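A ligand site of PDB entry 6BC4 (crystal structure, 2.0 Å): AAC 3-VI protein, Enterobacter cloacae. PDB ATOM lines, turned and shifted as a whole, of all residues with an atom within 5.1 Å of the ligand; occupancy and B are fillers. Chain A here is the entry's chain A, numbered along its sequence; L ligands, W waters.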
ATOM      1  N   PRO A  46      29.633 -17.320  -4.479  1.00  0.00           N
ATOM      2  CA  PRO A  46      28.657 -16.303  -4.880  1.00  0.00           C
ATOM      3  C   PRO A  46      28.939 -15.671  -6.235  1.00  0.00           C
ATOM      4  O   PRO A  46      30.083 -15.462  -6.647  1.00  0.00           O
ATOM      5  CB  PRO A  46      28.790 -15.263  -3.769  1.00  0.00           C
ATOM      6  CG  PRO A  46      30.228 -15.340  -3.376  1.00  0.00           C
ATOM      7  CD  PRO A  46      30.656 -16.782  -3.574  1.00  0.00           C
ATOM      8  N   HIS A  47      27.851 -15.367  -6.952  1.00  0.00           N
ATOM      9  CA  HIS A  47      27.872 -14.559  -8.165  1.00  0.00           C
ATOM     10  C   HIS A  47      26.871 -13.427  -7.945  1.00  0.00           C
ATOM     11  O   HIS A  47      25.663 -13.666  -7.894  1.00  0.00           O
ATOM     12  CB  HIS A  47      27.508 -15.383  -9.398  1.00  0.00           C
ATOM     13  CG  HIS A  47      28.459 -16.510  -9.677  1.00  0.00           C
ATOM     14  ND1 HIS A  47      29.734 -16.316 -10.141  1.00  0.00           N
ATOM     15  CD2 HIS A  47      28.310 -17.850  -9.539  1.00  0.00           C
ATOM     16  CE1 HIS A  47      30.339 -17.480 -10.287  1.00  0.00           C
ATOM     17  NE2 HIS A  47      29.488 -18.432  -9.926  1.00  0.00           N
ATOM     18  N   VAL A  48      27.370 -12.206  -7.810  1.00  0.00           N
ATOM     19  CA  VAL A  48      26.587 -11.100  -7.263  1.00  0.00           C
ATOM     20  C   VAL A  48      26.471  -9.972  -8.285  1.00  0.00           C
ATOM     21  O   VAL A  48      27.438  -9.636  -8.975  1.00  0.00           O
ATOM     22  CB  VAL A  48      27.221 -10.568  -5.952  1.00  0.00           C
ATOM     23  CG1 VAL A  48      26.364  -9.467  -5.356  1.00  0.00           C
ATOM     24  CG2 VAL A  48      27.415 -11.710  -4.967  1.00  0.00           C
ATOM     25  N   SER A  49      25.273  -9.401  -8.371  1.00  0.00           N
ATOM     26  CA  SER A  49      25.025  -8.133  -9.051  1.00  0.00           C
ATOM     27  C   SER A  49      24.680  -7.124  -7.956  1.00  0.00           C
ATOM     28  O   SER A  49      23.579  -7.147  -7.392  1.00  0.00           O
ATOM     29  CB  SER A  49      23.897  -8.257 -10.067  1.00  0.00           C
ATOM     30  OG  SER A  49      23.410  -6.985 -10.447  1.00  0.00           O
ATOM     31  N   LEU A  50      25.636  -6.247  -7.650  1.00  0.00           N
ATOM     32  CA  LEU A  50      25.433  -5.298  -6.552  1.00  0.00           C
ATOM     33  C   LEU A  50      24.317  -4.299  -6.865  1.00  0.00           C
ATOM     34  O   LEU A  50      23.672  -3.786  -5.939  1.00  0.00           O
ATOM     35  CB  LEU A  50      26.734  -4.558  -6.251  1.00  0.00           C
ATOM     36  CG  LEU A  50      27.764  -5.347  -5.429  1.00  0.00           C
ATOM     37  CD1 LEU A  50      29.081  -4.599  -5.344  1.00  0.00           C
ATOM     38  CD2 LEU A  50      27.211  -5.644  -4.045  1.00  0.00           C
ATOM     39  N   ARG A  51      24.080  -4.013  -8.138  1.00  0.00           N
ATOM     40  CA  ARG A  51      22.981  -3.120  -8.492  1.00  0.00           C
ATOM     41  C   ARG A  51      21.630  -3.771  -8.224  1.00  0.00           C
ATOM     42  O   ARG A  51      20.666  -3.078  -7.865  1.00  0.00           O
ATOM     43  CB  ARG A  51      23.095  -2.691  -9.956  1.00  0.00           C
ATOM     44  CG  ARG A  51      24.003  -1.494 -10.180  1.00  0.00           C
ATOM     45  CD  ARG A  51      24.633  -1.522 -11.553  1.00  0.00           C
ATOM     46  NE  ARG A  51      25.351  -0.283 -11.850  1.00  0.00           N
ATOM     47  CZ  ARG A  51      26.396  -0.211 -12.674  1.00  0.00           C
ATOM     48  NH1 ARG A  51      26.841  -1.293 -13.283  1.00  0.00           N
ATOM     49  NH2 ARG A  51      26.996   0.965 -12.888  1.00  0.00           N
ATOM     50  N   ALA A  52      21.535  -5.085  -8.394  1.00  0.00           N
ATOM     51  CA  ALA A  52      20.299  -5.779  -8.068  1.00  0.00           C
ATOM     52  C   ALA A  52      20.096  -5.881  -6.555  1.00  0.00           C
ATOM     53  O   ALA A  52      18.958  -5.897  -6.089  1.00  0.00           O
ATOM     54  CB  ALA A  52      20.282  -7.170  -8.702  1.00  0.00           C
ATOM     55  N   PRO A  60      29.296  -2.397  -0.329  1.00  0.00           N
ATOM     56  CA  PRO A  60      29.399  -3.835  -0.627  1.00  0.00           C
ATOM     57  C   PRO A  60      29.981  -4.654   0.506  1.00  0.00           C
ATOM     58  O   PRO A  60      29.753  -5.873   0.549  1.00  0.00           O
ATOM     59  CB  PRO A  60      30.290  -3.871  -1.879  1.00  0.00           C
ATOM     60  CG  PRO A  60      30.150  -2.517  -2.486  1.00  0.00           C
ATOM     61  CD  PRO A  60      29.988  -1.567  -1.342  1.00  0.00           C
ATOM     62  N   PHE A  80      35.387 -16.650  -7.958  1.00  0.00           N
ATOM     63  CA  PHE A  80      36.201 -16.529  -9.165  1.00  0.00           C
ATOM     64  C   PHE A  80      36.416 -15.042  -9.422  1.00  0.00           C
ATOM     65  O   PHE A  80      35.528 -14.358  -9.926  1.00  0.00           O
ATOM     66  CB  PHE A  80      35.534 -17.215 -10.347  1.00  0.00           C
ATOM     67  CG  PHE A  80      36.202 -16.948 -11.661  1.00  0.00           C
ATOM     68  CD1 PHE A  80      35.449 -16.662 -12.794  1.00  0.00           C
ATOM     69  CD2 PHE A  80      37.585 -16.980 -11.782  1.00  0.00           C
ATOM     70  CE1 PHE A  80      36.057 -16.422 -14.003  1.00  0.00           C
ATOM     71  CE2 PHE A  80      38.198 -16.726 -12.988  1.00  0.00           C
ATOM     72  CZ  PHE A  80      37.429 -16.445 -14.105  1.00  0.00           C
ATOM     73  N   PRO A 117      37.204  -6.377 -12.839  1.00  0.00           N
ATOM     74  CA  PRO A 117      35.960  -5.665 -12.500  1.00  0.00           C
ATOM     75  C   PRO A 117      34.730  -6.207 -13.212  1.00  0.00           C
ATOM     76  O   PRO A 117      33.614  -6.098 -12.679  1.00  0.00           O
ATOM     77  CB  PRO A 117      36.251  -4.215 -12.912  1.00  0.00           C
ATOM     78  CG  PRO A 117      37.753  -4.124 -12.976  1.00  0.00           C
ATOM     79  CD  PRO A 117      38.209  -5.480 -13.425  1.00  0.00           C
ATOM     80  N   GLY A 118      34.893  -6.800 -14.401  1.00  0.00           N
ATOM     81  CA  GLY A 118      33.758  -7.253 -15.171  1.00  0.00           C
ATOM     82  C   GLY A 118      32.976  -8.389 -14.542  1.00  0.00           C
ATOM     83  O   GLY A 118      31.833  -8.645 -14.935  1.00  0.00           O
ATOM     84  N   PHE A 119      33.572  -9.087 -13.567  1.00  0.00           N
ATOM     85  CA  PHE A 119      32.917 -10.198 -12.904  1.00  0.00           C
ATOM     86  C   PHE A 119      32.242  -9.791 -11.602  1.00  0.00           C
ATOM     87  O   PHE A 119      31.787 -10.655 -10.847  1.00  0.00           O
ATOM     88  CB  PHE A 119      33.923 -11.325 -12.635  1.00  0.00           C
ATOM     89  CG  PHE A 119      34.524 -11.911 -13.886  1.00  0.00           C
ATOM     90  CD1 PHE A 119      33.864 -11.811 -15.102  1.00  0.00           C
ATOM     91  CD2 PHE A 119      35.740 -12.565 -13.840  1.00  0.00           C
ATOM     92  CE1 PHE A 119      34.414 -12.344 -16.251  1.00  0.00           C
ATOM     93  CE2 PHE A 119      36.303 -13.103 -14.985  1.00  0.00           C
ATOM     94  CZ  PHE A 119      35.636 -12.994 -16.192  1.00  0.00           C
ATOM     95  N   GLY A 120      32.153  -8.491 -11.326  1.00  0.00           N
ATOM     96  CA  GLY A 120      31.454  -8.038 -10.115  1.00  0.00           C
ATOM     97  C   GLY A 120      32.391  -7.283  -9.187  1.00  0.00           C
ATOM     98  O   GLY A 120      33.476  -7.735  -8.848  1.00  0.00           O
ATOM     99  N   ALA A 121      31.932  -6.105  -8.758  1.00  0.00           N
ATOM    100  CA  ALA A 121      32.725  -5.272  -7.854  1.00  0.00           C
ATOM    101  C   ALA A 121      32.825  -5.879  -6.463  1.00  0.00           C
ATOM    102  O   ALA A 121      33.693  -5.463  -5.680  1.00  0.00           O
ATOM    103  CB  ALA A 121      32.125  -3.872  -7.769  1.00  0.00           C
ATOM    104  N   ILE A 122      31.979  -6.853  -6.122  1.00  0.00           N
ATOM    105  CA  ILE A 122      32.042  -7.484  -4.819  1.00  0.00           C
ATOM    106  C   ILE A 122      33.316  -8.300  -4.666  1.00  0.00           C
ATOM    107  O   ILE A 122      33.776  -8.527  -3.535  1.00  0.00           O
ATOM    108  CB  ILE A 122      30.796  -8.366  -4.579  1.00  0.00           C
ATOM    109  CG1 ILE A 122      30.653  -8.719  -3.101  1.00  0.00           C
ATOM    110  CG2 ILE A 122      30.852  -9.617  -5.435  1.00  0.00           C
ATOM    111  CD1 ILE A 122      30.161  -7.579  -2.251  1.00  0.00           C
ATOM    112  N   PHE A 125      36.205  -6.678  -2.869  1.00  0.00           N
ATOM    113  CA  PHE A 125      36.007  -6.686  -1.424  1.00  0.00           C
ATOM    114  C   PHE A 125      36.289  -8.058  -0.833  1.00  0.00           C
ATOM    115  O   PHE A 125      36.785  -8.161   0.295  1.00  0.00           O
ATOM    116  CB  PHE A 125      34.583  -6.236  -1.085  1.00  0.00           C
ATOM    117  CG  PHE A 125      34.329  -4.777  -1.356  1.00  0.00           C
ATOM    118  CD1 PHE A 125      34.494  -3.843  -0.355  1.00  0.00           C
ATOM    119  CD2 PHE A 125      33.905  -4.360  -2.602  1.00  0.00           C
ATOM    120  CE1 PHE A 125      34.256  -2.493  -0.593  1.00  0.00           C
ATOM    121  CE2 PHE A 125      33.661  -3.014  -2.853  1.00  0.00           C
ATOM    122  CZ  PHE A 125      33.839  -2.085  -1.848  1.00  0.00           C
ATOM    123  N   GLY A 182      21.100 -12.194  -7.924  1.00  0.00           N
ATOM    124  CA  GLY A 182      20.753 -11.267  -8.982  1.00  0.00           C
ATOM    125  C   GLY A 182      21.580 -11.386 -10.239  1.00  0.00           C
ATOM    126  O   GLY A 182      21.492 -10.515 -11.105  1.00  0.00           O
ATOM    127  N   ALA A 183      22.387 -12.441 -10.374  1.00  0.00           N
ATOM    128  CA  ALA A 183      23.232 -12.642 -11.544  1.00  0.00           C
ATOM    129  C   ALA A 183      22.535 -13.562 -12.536  1.00  0.00           C
ATOM    130  O   ALA A 183      21.716 -14.412 -12.169  1.00  0.00           O
ATOM    131  CB  ALA A 183      24.586 -13.223 -11.140  1.00  0.00           C
ATOM    132  N   GLY A 184      22.872 -13.390 -13.808  1.00  0.00           N
ATOM    133  CA  GLY A 184      22.288 -14.181 -14.861  1.00  0.00           C
ATOM    134  C   GLY A 184      22.839 -15.587 -14.899  1.00  0.00           C
ATOM    135  O   GLY A 184      23.844 -15.924 -14.265  1.00  0.00           O
ATOM    136  N   ASP A 186      24.489 -16.964 -17.099  1.00  0.00           N
ATOM    137  CA  ASP A 186      25.782 -17.044 -17.771  1.00  0.00           C
ATOM    138  C   ASP A 186      26.955 -17.026 -16.808  1.00  0.00           C
ATOM    139  O   ASP A 186      28.086 -17.281 -17.227  1.00  0.00           O
ATOM    140  CB  ASP A 186      25.920 -15.891 -18.758  1.00  0.00           C
ATOM    141  CG  ASP A 186      25.961 -14.539 -18.076  1.00  0.00           C
ATOM    142  OD1 ASP A 186      24.978 -14.203 -17.370  1.00  0.00           O
ATOM    143  OD2 ASP A 186      26.956 -13.811 -18.229  1.00  0.00           O
ATOM    144  N   ALA A 187      26.723 -16.736 -15.520  1.00  0.00           N
ATOM    145  CA  ALA A 187      27.790 -16.503 -14.572  1.00  0.00           C
ATOM    146  C   ALA A 187      28.241 -17.755 -13.832  1.00  0.00           C
ATOM    147  O   ALA A 187      29.150 -17.666 -12.999  1.00  0.00           O
ATOM    148  CB  ALA A 187      27.365 -15.438 -13.554  1.00  0.00           C
ATOM    149  N   VAL A 188      27.664 -18.915 -14.118  1.00  0.00           N
ATOM    150  CA  VAL A 188      27.978 -20.127 -13.370  1.00  0.00           C
ATOM    151  C   VAL A 188      29.355 -20.645 -13.749  1.00  0.00           C
ATOM    152  O   VAL A 188      29.498 -21.431 -14.701  1.00  0.00           O
ATOM    153  CB  VAL A 188      26.901 -21.211 -13.590  1.00  0.00           C
ATOM    154  CG1 VAL A 188      27.120 -22.379 -12.641  1.00  0.00           C
ATOM    155  CG2 VAL A 188      25.512 -20.619 -13.402  1.00  0.00           C
ATOM    156  N   THR A 189      30.384 -20.209 -13.017  1.00  0.00           N
ATOM    157  CA  THR A 189      31.755 -20.591 -13.328  1.00  0.00           C
ATOM    158  C   THR A 189      31.966 -22.104 -13.191  1.00  0.00           C
ATOM    159  O   THR A 189      32.748 -22.695 -13.946  1.00  0.00           O
ATOM    160  CB  THR A 189      32.729 -19.845 -12.429  1.00  0.00           C
ATOM    161  OG1 THR A 189      32.509 -18.432 -12.542  1.00  0.00           O
ATOM    162  CG2 THR A 189      34.173 -20.149 -12.817  1.00  0.00           C
ATOM    163  N   HIS A 192      32.217 -24.600 -16.114  1.00  0.00           N
ATOM    164  CA  HIS A 192      33.426 -24.782 -16.905  1.00  0.00           C
ATOM    165  C   HIS A 192      34.078 -26.135 -16.620  1.00  0.00           C
ATOM    166  O   HIS A 192      34.782 -26.672 -17.484  1.00  0.00           O
ATOM    167  CB  HIS A 192      34.421 -23.650 -16.615  1.00  0.00           C
ATOM    168  CG  HIS A 192      34.040 -22.345 -17.233  1.00  0.00           C
ATOM    169  ND1 HIS A 192      33.557 -22.241 -18.525  1.00  0.00           N
ATOM    170  CD2 HIS A 192      34.088 -21.075 -16.753  1.00  0.00           C
ATOM    171  CE1 HIS A 192      33.322 -20.971 -18.798  1.00  0.00           C
ATOM    172  NE2 HIS A 192      33.634 -20.242 -17.746  1.00  0.00           N
ATOM    173  N   VAL A 244      27.668 -22.289 -21.009  1.00  0.00           N
ATOM    174  CA  VAL A 244      27.320 -22.147 -19.597  1.00  0.00           C
ATOM    175  C   VAL A 244      25.896 -21.618 -19.456  1.00  0.00           C
ATOM    176  O   VAL A 244      25.093 -22.135 -18.666  1.00  0.00           O
ATOM    177  CB  VAL A 244      28.328 -21.239 -18.870  1.00  0.00           C
ATOM    178  CG1 VAL A 244      27.873 -20.977 -17.447  1.00  0.00           C
ATOM    179  CG2 VAL A 244      29.707 -21.873 -18.883  1.00  0.00           C
HETATM  180  N1  LIG L   1      32.984   0.572  -3.874  1.00  0.00           N
HETATM  181  C1  LIG L   1      31.631   0.799  -3.893  1.00  0.00           C
HETATM  182  N2  LIG L   1      30.933   0.595  -5.030  1.00  0.00           N
HETATM  183  C2  LIG L   1      31.563   0.175  -6.158  1.00  0.00           C
HETATM  184  C3  LIG L   1      32.887  -0.042  -6.138  1.00  0.00           C
HETATM  185  C4  LIG L   1      33.609   0.163  -4.971  1.00  0.00           C
HETATM  186  N3  LIG L   1      35.015   0.029  -4.581  1.00  0.00           N
HETATM  187  N4  LIG L   1      33.257  -0.442  -7.375  1.00  0.00           N
HETATM  188  C5  LIG L   1      32.159  -0.475  -8.143  1.00  0.00           C
HETATM  189  N5  LIG L   1      31.112  -0.085  -7.393  1.00  0.00           N
HETATM  190  C6  LIG L   1      29.761   0.039  -7.796  1.00  0.00           C
HETATM  191  C7  LIG L   1      29.637   0.486  -9.045  1.00  0.00           C
HETATM  192  O1  LIG L   1      29.883   1.929  -9.103  1.00  0.00           O
HETATM  193  C8  LIG L   1      28.152   0.163  -9.304  1.00  0.00           C
HETATM  194  O2  LIG L   1      27.410   1.036  -8.638  1.00  0.00           O
HETATM  195  P1  LIG L   1      26.545   2.156  -9.472  1.00  0.00           P
HETATM  196  O3  LIG L   1      26.462   3.401  -8.668  1.00  0.00           O
HETATM  197  O4  LIG L   1      27.244   2.464 -10.826  1.00  0.00           O
HETATM  198  O5  LIG L   1      25.111   1.615  -9.725  1.00  0.00           O
HETATM  199  C9  LIG L   1      27.979  -1.278  -8.650  1.00  0.00           C
HETATM  200  O6  LIG L   1      28.998  -1.438  -7.833  1.00  0.00           O
HETATM  201  C10 LIG L   1      28.009  -2.363  -9.708  1.00  0.00           C
HETATM  202  O7  LIG L   1      27.962  -3.600  -9.086  1.00  0.00           O
HETATM  203  P2  LIG L   1      28.512  -4.945  -9.936  1.00  0.00           P
HETATM  204  O8  LIG L   1      28.067  -6.191  -9.228  1.00  0.00           O
HETATM  205  O9  LIG L   1      30.014  -4.917  -9.981  1.00  0.00           O
HETATM  206  O10 LIG L   1      27.886  -4.916 -11.471  1.00  0.00           O
HETATM  207  P3  LIG L   1      26.203  -5.125 -11.814  1.00  0.00           P
HETATM  208  O11 LIG L   1      25.400  -4.908 -10.555  1.00  0.00           O
HETATM  209  O12 LIG L   1      25.755  -4.144 -12.883  1.00  0.00           O
HETATM  210  O13 LIG L   1      25.956  -6.708 -12.398  1.00  0.00           O
HETATM  211  C11 LIG L   1      27.314  -8.402 -13.327  1.00  0.00           C
HETATM  212  C12 LIG L   1      26.617  -7.074 -13.554  1.00  0.00           C
HETATM  213  C13 LIG L   1      28.545  -8.168 -12.418  1.00  0.00           C
HETATM  214  C14 LIG L   1      27.804  -8.973 -14.711  1.00  0.00           C
HETATM  215  C15 LIG L   1      26.314  -9.377 -12.658  1.00  0.00           C
HETATM  216  O14 LIG L   1      25.155  -9.410 -13.385  1.00  0.00           O
HETATM  217  C16 LIG L   1      26.931 -10.800 -12.601  1.00  0.00           C
HETATM  218  O15 LIG L   1      26.656 -11.613 -13.454  1.00  0.00           O
HETATM  219  N6  LIG L   1      27.835 -11.157 -11.504  1.00  0.00           N
HETATM  220  C17 LIG L   1      28.424 -12.474 -11.473  1.00  0.00           C
HETATM  221  C18 LIG L   1      29.533 -12.409 -12.529  1.00  0.00           C
HETATM  222  C19 LIG L   1      30.550 -13.602 -12.429  1.00  0.00           C
HETATM  223  O16 LIG L   1      30.684 -14.200 -11.428  1.00  0.00           O
HETATM  224  N7  LIG L   1      31.345 -13.927 -13.653  1.00  0.00           N
HETATM  225  C20 LIG L   1      32.331 -15.024 -13.655  1.00  0.00           C
HETATM  226  C21 LIG L   1      32.786 -15.237 -15.139  1.00  0.00           C
HETATM  227  S1  LIG L   1      31.455 -16.092 -16.038  1.00  0.00           S
HETATM  228  C22 LIG L   1      31.787 -17.869 -15.894  1.00  0.00           C
HETATM  229  O17 LIG L   1      32.760 -18.237 -15.324  1.00  0.00           O
HETATM  230  C23 LIG L   1      30.825 -18.886 -16.484  1.00  0.00           C
HETATM  231  O   HOH W   1      24.583 -11.960 -15.608  1.00  0.00           O
HETATM  232  O   HOH W   2      31.048   1.708 -11.762  1.00  0.00           O
HETATM  233  O   HOH W   3      29.255  -7.885  -7.750  1.00  0.00           O
HETATM  234  O   HOH W   4      34.516 -17.355 -17.665  1.00  0.00           O
HETATM  235  O   HOH W   5      32.879 -14.019  -9.716  1.00  0.00           O
HETATM  236  O   HOH W   6      27.916 -12.121 -16.327  1.00  0.00           O
HETATM  237  O   HOH W   7      30.337 -12.351 -16.112  1.00  0.00           O
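ND1 of His 47 lies within hydrogen-bond range of O16 of the ligand (2.7 Å). N6 of the ligand is in hydrogen-bond range of O of Val 48 (3.0 Å). An oxygen (O4) of the ligand is in salt-bridge range of the guanidinium group (NH2) of Arg 51 (2.6 Å). OG of Ser 49 sits at hydrogen-bond distance from O11 of the ligand (2.9 Å). The backbone NH (N) of Leu 50 sits at hydrogen-bond distance from an oxygen (O8) of the ligand. An oxygen (O9) of the ligand sits at hydrogen-bond distance from the backbone NH of Ala 121, 2.6 Å away. O17 of the ligand lies within hydrogen-bond range of NE2 of His 192, at 3.3 Å. OG1 of Thr 189 sits at hydrogen-bond distance from O17 of the ligand, 2.8 Å away. N of Arg 51 lies within hydrogen-bond range of O11 of the ligand, at 2.9 Å.
NE2 of His 47 lies close to O of Ala 187, 3.2 Å away. OG1 of Thr 189 is in hydrogen-bond range of O of Ala 187, 3.5 Å away. The side-chain hydroxyl (OG) of Ser 49 sits at hydrogen-bond distance from the backbone NH (N) of Ala 52 (3.4 Å).
The backbone carbonyl oxygen (O) of Asp 186 sits close to a sulfur (S1) of the ligand (3.8 Å). Residues that only touch the ligand: Pro 60 (3.8 Å), Phe 80 (3.6 Å), Phe 119 (3.3 Å), Gly 120 (3.4 Å), Phe 125 (3.4 Å), Ala 183 (3.5 Å), Ala 187 (3.8 Å), Val 188 (3.4 Å) and Val 244 (3.7 Å). Of the 25 residues printed, 18 come within 4 Å of the ligand. The nearest printed residue that does not touch the ligand is Gly 118 (4.05 Å).
Water W3 lies within hydrogen-bond range of O8 of the ligand (2.5 Å), O of Val 48 (2.8 Å), N of Ile 122 (3.3 Å) and N of Ala 121 (3.4 Å). Water W5 lies within hydrogen-bond range of the backbone carbonyl oxygen of Phe 80 (2.7 Å) and an oxygen (O16) of the ligand (2.8 Å). Water W1 lies within hydrogen-bond range of N of Gly 184, OD1 of Asp 186 and O15 of the ligand. Water W4 bridges NE2 of His 192 (3.0 Å) and O17 of the ligand (3.1 Å). Water W6 lies within hydrogen-bond range of OD2 of Asp 186 (2.7 Å) and O15 of the ligand (3.2 Å).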
